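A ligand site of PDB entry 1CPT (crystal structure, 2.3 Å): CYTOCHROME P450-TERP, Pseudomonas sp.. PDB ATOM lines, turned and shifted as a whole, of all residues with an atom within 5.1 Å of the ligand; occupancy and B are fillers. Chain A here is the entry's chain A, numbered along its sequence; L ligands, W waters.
CB of Leu 102 touches O4 of the ligand, 3.5 Å away. Thr 103 touches the ligand. CE2 of Phe 121 touches C26 of the ligand, at 3.7 Å. O of Ile 264 touches C25 of the ligand, 3.8 Å away. Ala 267 touches the ligand. CA of Gly 268 touches C21 of the ligand, 3.5 Å away. Thr 271 touches the ligand (OG1 to C16, 3.5 Å). OG1 of Thr 272 touches C18 of the ligand, 3.8 Å away. OG of Ser 275 touches C19 of the ligand, 3.6 Å away. CG1 of Val 308 touches C17 of the ligand, 3.8 Å away. Pro 313 touches the ligand (CG to C17, 3.5 Å). CG2 of Val 314 touches C2 of the ligand, 3.6 Å away. Phe 317 touches the ligand. OH of Tyr 342 touches O1 of the ligand (3.5 Å). O of Gly 369 touches C9 of the ligand, 3.5 Å away. CE2 of Phe 370 touches C15 of the ligand (3.7 Å). Gly 371 touches the ligand (CA to O2, 3.5 Å). N of Met 376 touches O2 of the ligand, 3.6 Å away. Leu 378 touches the ligand (CD2 to C31, 3.8 Å). Gly 379 touches the ligand. Leu 382 touches the ligand. Ala 383 touches the ligand (CB to C3, 3.9 Å). CE of Met 387 touches C19 of the ligand (3.4 Å). Hydrophobic or aromatic side chains within 4 Å of the ligand: Leu 102, His 110, Phe 121, Ala 267, Val 308, Pro 313, Val 314, Phe 317, Phe 370, His 375, Leu 378, Leu 382, Ala 383 and Met 387. Within 4 Å of the ligand: Leu 102, Thr 103, His 110, Arg 114, Phe 121, Ile 264, Ala 267, Gly 268, Thr 271, Thr 272, Ser 275, Val 308, Pro 313, Val 314, Phe 317, Arg 319, Tyr 342, Gly 369, Phe 370, Gly 371, Trp 372, His 375, Met 376, Cys 377, Leu 378, Gly 379, Leu 382, Ala 383 and Met 387. Along chain A the residues within 4 Å of the ligand span positions 102 to 387.
The backbone carbonyl oxygen (O) of Thr 271 is in hydrogen-bond range of the side-chain hydroxyl (OG) of Ser 275 (3.1 Å). The side-chain sulfur (SG) of Cys 377 lies close to the backbone NH (N) of Gln 380, at 3.5 Å. The side-chain sulfur (SD) of Met 376 lies within hydrogen-bond range of the side-chain amide nitrogen (NE2) of Gln 380 (3.4 Å). ND1 of His 375 lies close to O of Leu 102 (3.4 Å). A ring nitrogen (ND1) of His 375 sits at hydrogen-bond distance from a ring nitrogen (NE2) of His 110 (3.4 Å). The side-chain hydroxyl (OG1) of Thr 272 lies within hydrogen-bond range of the backbone carbonyl oxygen (O) of Gly 268 (3.1 Å). The guanidinium group (NH1) of Arg 114 lies within hydrogen-bond range of the backbone carbonyl oxygen (O) of Met 376, at 2.8 Å. The side-chain sulfur (SG) of Cys 377 lies close to the backbone NH (N) of Gly 379.
Water W1 lies within hydrogen-bond range of OH of Tyr 342 and O2 of the ligand. Water W2 lies within hydrogen-bond range of an oxygen (O1) of the ligand (2.9 Å) and the guanidinium group (NH1) of Arg 319 (3.4 Å).
The backbone NH (N) of Trp 372 lies within hydrogen-bond range of an oxygen (O2) of the ligand, at 3.3 Å. The side-chain sulfur (SG) of Cys 377 binds an iron atom (FE1) of the ligand, at 2.1 Å. A ring nitrogen (NE2) of His 110 sits at hydrogen-bond distance from an oxygen (O3) of the ligand, at 2.7 Å. An oxygen (O4) of the ligand sits at hydrogen-bond distance from a ring nitrogen (ND1) of His 375 (2.7 Å). An oxygen (O1) of the ligand lies within salt-bridge range of the guanidinium group of Arg 319. The guanidinium group (NH1) of Arg 114 is in salt-bridge range of an oxygen (O3) of the ligand.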
ATOM      1  N   LEU A 102      38.409   6.956 -22.790  1.00  0.00           N
ATOM      2  CA  LEU A 102      37.464   6.737 -21.701  1.00  0.00           C
ATOM      3  C   LEU A 102      36.491   5.595 -21.945  1.00  0.00           C
ATOM      4  O   LEU A 102      36.196   4.872 -20.995  1.00  0.00           O
ATOM      5  CB  LEU A 102      36.676   8.035 -21.439  1.00  0.00           C
ATOM      6  CG  LEU A 102      37.444   9.339 -21.126  1.00  0.00           C
ATOM      7  CD1 LEU A 102      36.461  10.397 -20.781  1.00  0.00           C
ATOM      8  CD2 LEU A 102      38.367   9.229 -19.933  1.00  0.00           C
ATOM      9  N   THR A 103      36.072   5.278 -23.175  1.00  0.00           N
ATOM     10  CA  THR A 103      35.053   4.238 -23.337  1.00  0.00           C
ATOM     11  C   THR A 103      35.596   2.853 -23.230  1.00  0.00           C
ATOM     12  O   THR A 103      34.846   1.873 -23.114  1.00  0.00           O
ATOM     13  CB  THR A 103      34.295   4.365 -24.691  1.00  0.00           C
ATOM     14  OG1 THR A 103      35.231   4.586 -25.756  1.00  0.00           O
ATOM     15  CG2 THR A 103      33.256   5.475 -24.596  1.00  0.00           C
ATOM     16  N   HIS A 110      39.092   4.549 -15.264  1.00  0.00           N
ATOM     17  CA  HIS A 110      38.137   5.425 -15.918  1.00  0.00           C
ATOM     18  C   HIS A 110      37.845   6.626 -15.048  1.00  0.00           C
ATOM     19  O   HIS A 110      37.774   7.722 -15.607  1.00  0.00           O
ATOM     20  CB  HIS A 110      36.826   4.653 -16.222  1.00  0.00           C
ATOM     21  CG  HIS A 110      35.661   5.537 -16.700  1.00  0.00           C
ATOM     22  ND1 HIS A 110      34.559   5.984 -16.066  1.00  0.00           N
ATOM     23  CD2 HIS A 110      35.713   6.195 -17.897  1.00  0.00           C
ATOM     24  CE1 HIS A 110      33.971   6.870 -16.816  1.00  0.00           C
ATOM     25  NE2 HIS A 110      34.675   6.990 -17.904  1.00  0.00           N
ATOM     26  N   ARG A 114      38.743  10.227 -16.559  1.00  0.00           N
ATOM     27  CA  ARG A 114      37.602  11.101 -16.770  1.00  0.00           C
ATOM     28  C   ARG A 114      37.680  12.363 -15.887  1.00  0.00           C
ATOM     29  O   ARG A 114      37.320  13.534 -16.208  1.00  0.00           O
ATOM     30  CB  ARG A 114      36.356  10.221 -16.519  1.00  0.00           C
ATOM     31  CG  ARG A 114      35.061  10.965 -16.847  1.00  0.00           C
ATOM     32  CD  ARG A 114      33.831  10.095 -16.687  1.00  0.00           C
ATOM     33  NE  ARG A 114      32.661  10.961 -16.591  1.00  0.00           N
ATOM     34  CZ  ARG A 114      31.595  10.974 -17.434  1.00  0.00           C
ATOM     35  NH1 ARG A 114      31.518  10.163 -18.495  1.00  0.00           N
ATOM     36  NH2 ARG A 114      30.613  11.870 -17.234  1.00  0.00           N
ATOM     37  N   PHE A 121      34.371  20.413 -18.511  1.00  0.00           N
ATOM     38  CA  PHE A 121      33.139  20.144 -19.239  1.00  0.00           C
ATOM     39  C   PHE A 121      31.864  20.495 -18.470  1.00  0.00           C
ATOM     40  O   PHE A 121      30.763  20.393 -19.019  1.00  0.00           O
ATOM     41  CB  PHE A 121      33.132  18.663 -19.650  1.00  0.00           C
ATOM     42  CG  PHE A 121      34.101  18.507 -20.800  1.00  0.00           C
ATOM     43  CD1 PHE A 121      35.357  17.990 -20.585  1.00  0.00           C
ATOM     44  CD2 PHE A 121      33.750  18.970 -22.048  1.00  0.00           C
ATOM     45  CE1 PHE A 121      36.285  17.940 -21.615  1.00  0.00           C
ATOM     46  CE2 PHE A 121      34.685  18.921 -23.072  1.00  0.00           C
ATOM     47  CZ  PHE A 121      35.949  18.404 -22.850  1.00  0.00           C
ATOM     48  N   VAL A 166      34.604  22.050 -31.347  1.00  0.00           N
ATOM     49  CA  VAL A 166      35.509  21.133 -30.694  1.00  0.00           C
ATOM     50  C   VAL A 166      36.981  21.529 -30.988  1.00  0.00           C
ATOM     51  O   VAL A 166      37.865  21.419 -30.118  1.00  0.00           O
ATOM     52  CB  VAL A 166      34.964  19.722 -31.187  1.00  0.00           C
ATOM     53  CG1 VAL A 166      35.582  19.200 -32.440  1.00  0.00           C
ATOM     54  CG2 VAL A 166      35.264  18.750 -30.095  1.00  0.00           C
ATOM     55  N   ALA A 263      39.427  11.012 -28.897  1.00  0.00           N
ATOM     56  CA  ALA A 263      38.133  10.661 -28.373  1.00  0.00           C
ATOM     57  C   ALA A 263      37.296  11.916 -28.360  1.00  0.00           C
ATOM     58  O   ALA A 263      36.216  11.877 -28.908  1.00  0.00           O
ATOM     59  CB  ALA A 263      38.315  10.139 -26.984  1.00  0.00           C
ATOM     60  N   ILE A 264      37.714  13.076 -27.854  1.00  0.00           N
ATOM     61  CA  ILE A 264      36.858  14.258 -27.814  1.00  0.00           C
ATOM     62  C   ILE A 264      36.388  14.715 -29.214  1.00  0.00           C
ATOM     63  O   ILE A 264      35.185  14.799 -29.543  1.00  0.00           O
ATOM     64  CB  ILE A 264      37.681  15.319 -27.041  1.00  0.00           C
ATOM     65  CG1 ILE A 264      37.638  14.950 -25.547  1.00  0.00           C
ATOM     66  CG2 ILE A 264      37.166  16.742 -27.268  1.00  0.00           C
ATOM     67  CD1 ILE A 264      38.542  15.964 -24.766  1.00  0.00           C
ATOM     68  N   ALA A 267      34.149  12.089 -30.915  1.00  0.00           N
ATOM     69  CA  ALA A 267      32.927  11.890 -30.163  1.00  0.00           C
ATOM     70  C   ALA A 267      32.055  13.114 -30.241  1.00  0.00           C
ATOM     71  O   ALA A 267      30.817  13.039 -30.124  1.00  0.00           O
ATOM     72  CB  ALA A 267      33.241  11.626 -28.720  1.00  0.00           C
ATOM     73  N   GLY A 268      32.707  14.233 -30.458  1.00  0.00           N
ATOM     74  CA  GLY A 268      31.995  15.475 -30.503  1.00  0.00           C
ATOM     75  C   GLY A 268      31.643  15.951 -31.896  1.00  0.00           C
ATOM     76  O   GLY A 268      30.981  16.996 -31.975  1.00  0.00           O
ATOM     77  N   THR A 271      27.958  13.363 -33.740  1.00  0.00           N
ATOM     78  CA  THR A 271      26.782  13.351 -32.879  1.00  0.00           C
ATOM     79  C   THR A 271      26.146  14.760 -32.904  1.00  0.00           C
ATOM     80  O   THR A 271      24.935  14.917 -33.086  1.00  0.00           O
ATOM     81  CB  THR A 271      27.307  12.918 -31.511  1.00  0.00           C
ATOM     82  OG1 THR A 271      28.332  13.848 -31.184  1.00  0.00           O
ATOM     83  CG2 THR A 271      27.832  11.512 -31.486  1.00  0.00           C
ATOM     84  N   THR A 272      26.920  15.831 -32.837  1.00  0.00           N
ATOM     85  CA  THR A 272      26.308  17.143 -32.805  1.00  0.00           C
ATOM     86  C   THR A 272      25.789  17.573 -34.150  1.00  0.00           C
ATOM     87  O   THR A 272      24.658  18.078 -34.175  1.00  0.00           O
ATOM     88  CB  THR A 272      27.333  18.118 -32.235  1.00  0.00           C
ATOM     89  OG1 THR A 272      27.995  17.351 -31.225  1.00  0.00           O
ATOM     90  CG2 THR A 272      26.734  19.399 -31.647  1.00  0.00           C
ATOM     91  N   SER A 275      22.442  15.485 -34.784  1.00  0.00           N
ATOM     92  CA  SER A 275      21.366  16.082 -34.032  1.00  0.00           C
ATOM     93  C   SER A 275      20.918  17.423 -34.554  1.00  0.00           C
ATOM     94  O   SER A 275      19.718  17.694 -34.438  1.00  0.00           O
ATOM     95  CB  SER A 275      21.769  16.299 -32.585  1.00  0.00           C
ATOM     96  OG  SER A 275      22.014  15.021 -32.060  1.00  0.00           O
ATOM     97  N   VAL A 308      17.987  15.706 -30.016  1.00  0.00           N
ATOM     98  CA  VAL A 308      18.828  14.598 -29.568  1.00  0.00           C
ATOM     99  C   VAL A 308      17.930  13.442 -29.175  1.00  0.00           C
ATOM    100  O   VAL A 308      18.347  12.303 -29.354  1.00  0.00           O
ATOM    101  CB  VAL A 308      19.660  15.009 -28.373  1.00  0.00           C
ATOM    102  CG1 VAL A 308      20.607  13.910 -28.023  1.00  0.00           C
ATOM    103  CG2 VAL A 308      20.386  16.295 -28.670  1.00  0.00           C
ATOM    104  N   PRO A 313      21.524   9.865 -32.249  1.00  0.00           N
ATOM    105  CA  PRO A 313      22.611   9.566 -33.173  1.00  0.00           C
ATOM    106  C   PRO A 313      23.463   8.367 -32.786  1.00  0.00           C
ATOM    107  O   PRO A 313      23.905   7.609 -33.641  1.00  0.00           O
ATOM    108  CB  PRO A 313      23.357  10.908 -33.264  1.00  0.00           C
ATOM    109  CG  PRO A 313      23.016  11.650 -31.976  1.00  0.00           C
ATOM    110  CD  PRO A 313      21.586  11.249 -31.783  1.00  0.00           C
ATOM    111  N   VAL A 314      23.728   8.105 -31.496  1.00  0.00           N
ATOM    112  CA  VAL A 314      24.469   6.938 -31.052  1.00  0.00           C
ATOM    113  C   VAL A 314      23.424   5.853 -30.935  1.00  0.00           C
ATOM    114  O   VAL A 314      22.535   5.872 -30.089  1.00  0.00           O
ATOM    115  CB  VAL A 314      25.141   7.187 -29.703  1.00  0.00           C
ATOM    116  CG1 VAL A 314      25.932   5.963 -29.292  1.00  0.00           C
ATOM    117  CG2 VAL A 314      26.054   8.377 -29.794  1.00  0.00           C
ATOM    118  N   PHE A 317      26.042   1.083 -27.666  1.00  0.00           N
ATOM    119  CA  PHE A 317      27.344   0.853 -27.079  1.00  0.00           C
ATOM    120  C   PHE A 317      27.202  -0.521 -26.456  1.00  0.00           C
ATOM    121  O   PHE A 317      26.075  -0.998 -26.270  1.00  0.00           O
ATOM    122  CB  PHE A 317      27.662   1.795 -25.979  1.00  0.00           C
ATOM    123  CG  PHE A 317      28.571   2.900 -26.450  1.00  0.00           C
ATOM    124  CD1 PHE A 317      28.137   4.206 -26.445  1.00  0.00           C
ATOM    125  CD2 PHE A 317      29.863   2.630 -26.838  1.00  0.00           C
ATOM    126  CE1 PHE A 317      29.016   5.211 -26.831  1.00  0.00           C
ATOM    127  CE2 PHE A 317      30.712   3.635 -27.221  1.00  0.00           C
ATOM    128  CZ  PHE A 317      30.291   4.931 -27.228  1.00  0.00           C
ATOM    129  N   ARG A 319      28.292  -3.726 -23.527  1.00  0.00           N
ATOM    130  CA  ARG A 319      28.688  -4.029 -22.152  1.00  0.00           C
ATOM    131  C   ARG A 319      28.925  -5.505 -22.050  1.00  0.00           C
ATOM    132  O   ARG A 319      28.264  -6.265 -22.776  1.00  0.00           O
ATOM    133  CB  ARG A 319      27.619  -3.680 -21.135  1.00  0.00           C
ATOM    134  CG  ARG A 319      27.358  -2.207 -20.892  1.00  0.00           C
ATOM    135  CD  ARG A 319      28.612  -1.404 -20.590  1.00  0.00           C
ATOM    136  NE  ARG A 319      28.265  -0.030 -20.203  1.00  0.00           N
ATOM    137  CZ  ARG A 319      28.338   1.051 -20.984  1.00  0.00           C
ATOM    138  NH1 ARG A 319      28.739   1.030 -22.249  1.00  0.00           N
ATOM    139  NH2 ARG A 319      28.104   2.230 -20.435  1.00  0.00           N
ATOM    140  N   TYR A 342      20.110   3.016 -27.235  1.00  0.00           N
ATOM    141  CA  TYR A 342      19.639   4.340 -26.901  1.00  0.00           C
ATOM    142  C   TYR A 342      18.456   4.699 -27.789  1.00  0.00           C
ATOM    143  O   TYR A 342      17.488   5.138 -27.192  1.00  0.00           O
ATOM    144  CB  TYR A 342      20.762   5.363 -27.066  1.00  0.00           C
ATOM    145  CG  TYR A 342      21.973   4.939 -26.245  1.00  0.00           C
ATOM    146  CD1 TYR A 342      23.104   4.442 -26.891  1.00  0.00           C
ATOM    147  CD2 TYR A 342      21.948   4.972 -24.869  1.00  0.00           C
ATOM    148  CE1 TYR A 342      24.183   3.964 -26.160  1.00  0.00           C
ATOM    149  CE2 TYR A 342      23.027   4.494 -24.138  1.00  0.00           C
ATOM    150  CZ  TYR A 342      24.121   3.996 -24.788  1.00  0.00           C
ATOM    151  OH  TYR A 342      25.181   3.506 -24.050  1.00  0.00           O
ATOM    152  N   GLY A 369      19.714   9.873 -24.728  1.00  0.00           N
ATOM    153  CA  GLY A 369      20.480  10.189 -25.915  1.00  0.00           C
ATOM    154  C   GLY A 369      21.949  10.346 -25.614  1.00  0.00           C
ATOM    155  O   GLY A 369      22.722   9.965 -26.477  1.00  0.00           O
ATOM    156  N   PHE A 370      22.327  10.846 -24.447  1.00  0.00           N
ATOM    157  CA  PHE A 370      23.680  11.043 -23.999  1.00  0.00           C
ATOM    158  C   PHE A 370      24.022   9.909 -23.095  1.00  0.00           C
ATOM    159  O   PHE A 370      25.014  10.024 -22.404  1.00  0.00           O
ATOM    160  CB  PHE A 370      23.887  12.341 -23.212  1.00  0.00           C
ATOM    161  CG  PHE A 370      23.631  13.656 -23.963  1.00  0.00           C
ATOM    162  CD1 PHE A 370      22.412  14.304 -23.850  1.00  0.00           C
ATOM    163  CD2 PHE A 370      24.597  14.196 -24.800  1.00  0.00           C
ATOM    164  CE1 PHE A 370      22.158  15.447 -24.571  1.00  0.00           C
ATOM    165  CE2 PHE A 370      24.336  15.338 -25.528  1.00  0.00           C
ATOM    166  CZ  PHE A 370      23.122  15.981 -25.421  1.00  0.00           C
ATOM    167  N   GLY A 371      23.265   8.824 -23.033  1.00  0.00           N
ATOM    168  CA  GLY A 371      23.568   7.700 -22.162  1.00  0.00           C
ATOM    169  C   GLY A 371      23.108   8.009 -20.749  1.00  0.00           C
ATOM    170  O   GLY A 371      22.396   8.987 -20.491  1.00  0.00           O
ATOM    171  N   TRP A 372      23.562   7.186 -19.791  1.00  0.00           N
ATOM    172  CA  TRP A 372      23.192   7.283 -18.392  1.00  0.00           C
ATOM    173  C   TRP A 372      24.158   6.416 -17.634  1.00  0.00           C
ATOM    174  O   TRP A 372      24.443   5.254 -17.963  1.00  0.00           O
ATOM    175  CB  TRP A 372      21.765   6.729 -18.101  1.00  0.00           C
ATOM    176  CG  TRP A 372      21.196   7.128 -16.727  1.00  0.00           C
ATOM    177  CD1 TRP A 372      21.294   6.290 -15.626  1.00  0.00           C
ATOM    178  CD2 TRP A 372      20.636   8.360 -16.408  1.00  0.00           C
ATOM    179  NE1 TRP A 372      20.823   7.014 -14.621  1.00  0.00           N
ATOM    180  CE2 TRP A 372      20.440   8.230 -15.038  1.00  0.00           C
ATOM    181  CE3 TRP A 372      20.300   9.535 -17.074  1.00  0.00           C
ATOM    182  CZ2 TRP A 372      19.889   9.273 -14.302  1.00  0.00           C
ATOM    183  CZ3 TRP A 372      19.740  10.574 -16.328  1.00  0.00           C
ATOM    184  CH2 TRP A 372      19.537  10.449 -14.952  1.00  0.00           C
ATOM    185  N   GLY A 373      24.732   6.969 -16.576  1.00  0.00           N
ATOM    186  CA  GLY A 373      25.643   6.168 -15.796  1.00  0.00           C
ATOM    187  C   GLY A 373      27.017   6.749 -15.699  1.00  0.00           C
ATOM    188  O   GLY A 373      27.193   7.976 -15.848  1.00  0.00           O
ATOM    189  N   ALA A 374      27.975   5.823 -15.466  1.00  0.00           N
ATOM    190  CA  ALA A 374      29.387   6.191 -15.300  1.00  0.00           C
ATOM    191  C   ALA A 374      29.979   6.904 -16.518  1.00  0.00           C
ATOM    192  O   ALA A 374      30.725   7.877 -16.383  1.00  0.00           O
ATOM    193  CB  ALA A 374      30.270   4.980 -15.088  1.00  0.00           C
ATOM    194  N   HIS A 375      29.685   6.356 -17.725  1.00  0.00           N
ATOM    195  CA  HIS A 375      30.184   6.887 -19.003  1.00  0.00           C
ATOM    196  C   HIS A 375      29.322   7.986 -19.632  1.00  0.00           C
ATOM    197  O   HIS A 375      29.540   8.340 -20.784  1.00  0.00           O
ATOM    198  CB  HIS A 375      30.382   5.735 -20.012  1.00  0.00           C
ATOM    199  CG  HIS A 375      31.619   4.910 -19.674  1.00  0.00           C
ATOM    200  ND1 HIS A 375      32.923   4.946 -19.973  1.00  0.00           N
ATOM    201  CD2 HIS A 375      31.536   3.863 -18.783  1.00  0.00           C
ATOM    202  CE1 HIS A 375      33.597   4.005 -19.322  1.00  0.00           C
ATOM    203  NE2 HIS A 375      32.739   3.360 -18.602  1.00  0.00           N
ATOM    204  N   MET A 376      28.377   8.590 -18.917  1.00  0.00           N
ATOM    205  CA  MET A 376      27.462   9.484 -19.528  1.00  0.00           C
ATOM    206  C   MET A 376      28.249  10.579 -20.233  1.00  0.00           C
ATOM    207  O   MET A 376      29.182  11.087 -19.665  1.00  0.00           O
ATOM    208  CB  MET A 376      26.579  10.051 -18.452  1.00  0.00           C
ATOM    209  CG  MET A 376      25.297  10.608 -19.093  1.00  0.00           C
ATOM    210  SD  MET A 376      24.089  11.509 -18.117  1.00  0.00           S
ATOM    211  CE  MET A 376      23.948  10.336 -16.847  1.00  0.00           C
ATOM    212  N   CYS A 377      27.891  10.930 -21.478  1.00  0.00           N
ATOM    213  CA  CYS A 377      28.578  11.820 -22.348  1.00  0.00           C
ATOM    214  C   CYS A 377      29.185  13.017 -21.696  1.00  0.00           C
ATOM    215  O   CYS A 377      28.541  13.948 -21.243  1.00  0.00           O
ATOM    216  CB  CYS A 377      27.666  12.311 -23.417  1.00  0.00           C
ATOM    217  SG  CYS A 377      28.470  13.377 -24.662  1.00  0.00           S
ATOM    218  N   LEU A 378      30.502  12.964 -21.607  1.00  0.00           N
ATOM    219  CA  LEU A 378      31.280  14.043 -21.078  1.00  0.00           C
ATOM    220  C   LEU A 378      30.966  15.387 -21.713  1.00  0.00           C
ATOM    221  O   LEU A 378      30.884  16.419 -21.017  1.00  0.00           O
ATOM    222  CB  LEU A 378      32.716  13.659 -21.256  1.00  0.00           C
ATOM    223  CG  LEU A 378      33.773  14.604 -20.776  1.00  0.00           C
ATOM    224  CD1 LEU A 378      33.792  14.731 -19.266  1.00  0.00           C
ATOM    225  CD2 LEU A 378      35.082  14.040 -21.282  1.00  0.00           C
ATOM    226  N   GLY A 379      30.644  15.356 -23.001  1.00  0.00           N
ATOM    227  CA  GLY A 379      30.430  16.575 -23.727  1.00  0.00           C
ATOM    228  C   GLY A 379      28.985  17.016 -23.706  1.00  0.00           C
ATOM    229  O   GLY A 379      28.747  18.041 -24.345  1.00  0.00           O
ATOM    230  N   GLN A 380      28.032  16.427 -22.964  1.00  0.00           N
ATOM    231  CA  GLN A 380      26.624  16.850 -23.024  1.00  0.00           C
ATOM    232  C   GLN A 380      26.312  18.299 -22.798  1.00  0.00           C
ATOM    233  O   GLN A 380      25.417  18.858 -23.440  1.00  0.00           O
ATOM    234  CB  GLN A 380      25.766  16.043 -22.084  1.00  0.00           C
ATOM    235  CG  GLN A 380      26.016  16.207 -20.617  1.00  0.00           C
ATOM    236  CD  GLN A 380      24.945  15.552 -19.759  1.00  0.00           C
ATOM    237  OE1 GLN A 380      23.783  15.965 -19.756  1.00  0.00           O
ATOM    238  NE2 GLN A 380      25.308  14.550 -18.978  1.00  0.00           N
ATOM    239  N   LEU A 382      28.513  20.874 -23.320  1.00  0.00           N
ATOM    240  CA  LEU A 382      29.079  21.565 -24.480  1.00  0.00           C
ATOM    241  C   LEU A 382      28.143  21.318 -25.653  1.00  0.00           C
ATOM    242  O   LEU A 382      27.768  22.289 -26.288  1.00  0.00           O
ATOM    243  CB  LEU A 382      30.536  21.018 -24.765  1.00  0.00           C
ATOM    244  CG  LEU A 382      31.216  21.627 -26.038  1.00  0.00           C
ATOM    245  CD1 LEU A 382      31.231  23.166 -25.916  1.00  0.00           C
ATOM    246  CD2 LEU A 382      32.600  20.985 -26.236  1.00  0.00           C
ATOM    247  N   ALA A 383      27.670  20.104 -25.921  1.00  0.00           N
ATOM    248  CA  ALA A 383      26.756  19.788 -26.979  1.00  0.00           C
ATOM    249  C   ALA A 383      25.470  20.538 -26.822  1.00  0.00           C
ATOM    250  O   ALA A 383      24.975  21.065 -27.823  1.00  0.00           O
ATOM    251  CB  ALA A 383      26.385  18.336 -27.010  1.00  0.00           C
ATOM    252  N   GLU A 386      26.411  24.627 -27.568  1.00  0.00           N
ATOM    253  CA  GLU A 386      26.630  24.962 -28.953  1.00  0.00           C
ATOM    254  C   GLU A 386      25.400  24.635 -29.779  1.00  0.00           C
ATOM    255  O   GLU A 386      25.257  25.330 -30.775  1.00  0.00           O
ATOM    256  CB  GLU A 386      27.807  24.194 -29.474  1.00  0.00           C
ATOM    257  CG  GLU A 386      27.564  22.725 -29.740  1.00  0.00           C
ATOM    258  CD  GLU A 386      28.747  21.988 -30.314  1.00  0.00           C
ATOM    259  OE1 GLU A 386      29.182  20.984 -29.755  1.00  0.00           O
ATOM    260  OE2 GLU A 386      29.238  22.403 -31.353  1.00  0.00           O
ATOM    261  N   MET A 387      24.493  23.652 -29.541  1.00  0.00           N
ATOM    262  CA  MET A 387      23.316  23.530 -30.385  1.00  0.00           C
ATOM    263  C   MET A 387      22.344  24.661 -30.073  1.00  0.00           C
ATOM    264  O   MET A 387      21.770  25.264 -30.970  1.00  0.00           O
ATOM    265  CB  MET A 387      22.596  22.221 -30.180  1.00  0.00           C
ATOM    266  CG  MET A 387      23.370  21.051 -30.746  1.00  0.00           C
ATOM    267  SD  MET A 387      22.398  19.556 -30.926  1.00  0.00           S
ATOM    268  CE  MET A 387      23.116  18.908 -29.477  1.00  0.00           C
HETATM  269  C1  LIG L   1      30.132   9.313 -24.764  1.00  0.00           C
HETATM  270  C2  LIG L   1      26.230  10.783 -27.107  1.00  0.00           C
HETATM  271  C3  LIG L   1      28.268  15.043 -27.846  1.00  0.00           C
HETATM  272  C4  LIG L   1      32.318  13.454 -25.866  1.00  0.00           C
HETATM  273  C5  LIG L   1      28.819   9.404 -25.212  1.00  0.00           C
HETATM  274  C6  LIG L   1      27.840   8.308 -25.119  1.00  0.00           C
HETATM  275  C7  LIG L   1      26.768   8.719 -25.837  1.00  0.00           C
HETATM  276  C8  LIG L   1      27.061  10.083 -26.296  1.00  0.00           C
HETATM  277  C9  LIG L   1      25.515   7.903 -26.094  1.00  0.00           C
HETATM  278  C10 LIG L   1      27.897   7.033 -24.308  1.00  0.00           C
HETATM  279  C11 LIG L   1      27.422   7.277 -22.873  1.00  0.00           C
HETATM  280  C12 LIG L   1      27.215   6.107 -21.940  1.00  0.00           C
HETATM  281  O1  LIG L   1      27.741   5.039 -22.183  1.00  0.00           O
HETATM  282  O2  LIG L   1      26.519   6.228 -20.929  1.00  0.00           O
HETATM  283  C13 LIG L   1      26.472  12.061 -27.563  1.00  0.00           C
HETATM  284  C14 LIG L   1      25.492  12.874 -28.273  1.00  0.00           C
HETATM  285  C15 LIG L   1      26.064  14.069 -28.485  1.00  0.00           C
HETATM  286  C16 LIG L   1      27.356  13.994 -27.873  1.00  0.00           C
HETATM  287  C17 LIG L   1      24.086  12.427 -28.698  1.00  0.00           C
HETATM  288  C18 LIG L   1      25.597  15.145 -29.237  1.00  0.00           C
HETATM  289  C19 LIG L   1      24.280  15.728 -29.336  1.00  0.00           C
HETATM  290  C20 LIG L   1      29.566  14.991 -27.330  1.00  0.00           C
HETATM  291  C21 LIG L   1      30.516  16.093 -27.407  1.00  0.00           C
HETATM  292  C22 LIG L   1      31.677  15.616 -26.908  1.00  0.00           C
HETATM  293  C23 LIG L   1      31.408  14.243 -26.501  1.00  0.00           C
HETATM  294  C24 LIG L   1      30.201  17.473 -27.942  1.00  0.00           C
HETATM  295  C25 LIG L   1      32.932  16.208 -26.877  1.00  0.00           C
HETATM  296  C26 LIG L   1      33.276  17.446 -26.213  1.00  0.00           C
HETATM  297  C27 LIG L   1      32.042  12.223 -25.335  1.00  0.00           C
HETATM  298  C28 LIG L   1      33.015  11.438 -24.622  1.00  0.00           C
HETATM  299  C29 LIG L   1      32.393  10.300 -24.275  1.00  0.00           C
HETATM  300  C30 LIG L   1      31.055  10.357 -24.837  1.00  0.00           C
HETATM  301  C31 LIG L   1      34.461  11.788 -24.273  1.00  0.00           C
HETATM  302  C32 LIG L   1      33.005   9.216 -23.384  1.00  0.00           C
HETATM  303  C33 LIG L   1      32.743   9.434 -21.893  1.00  0.00           C
HETATM  304  C34 LIG L   1      33.222   8.279 -21.030  1.00  0.00           C
HETATM  305  O3  LIG L   1      33.535   8.530 -19.871  1.00  0.00           O
HETATM  306  O4  LIG L   1      33.309   7.134 -21.443  1.00  0.00           O
HETATM  307  N1  LIG L   1      28.311  10.504 -25.893  1.00  0.00           N
HETATM  308  N2  LIG L   1      27.618  12.751 -27.310  1.00  0.00           N
HETATM  309  N3  LIG L   1      30.103  13.867 -26.749  1.00  0.00           N
HETATM  310  N4  LIG L   1      30.833  11.573 -25.453  1.00  0.00           N
HETATM  311 FE1  LIG L   1      29.193  12.203 -26.308  1.00  0.00          FE
HETATM  312  O   HOH W   1      24.939   4.058 -21.420  1.00  0.00           O
HETATM  313  O   HOH W   2      30.076   3.932 -23.437  1.00  0.00           O
HETATM  314  O   HOH W   3      29.834  11.179 -28.015  1.00  0.00           O
HETATM  315  O   HOH W   4      27.394   4.765 -18.603  1.00  0.00           O
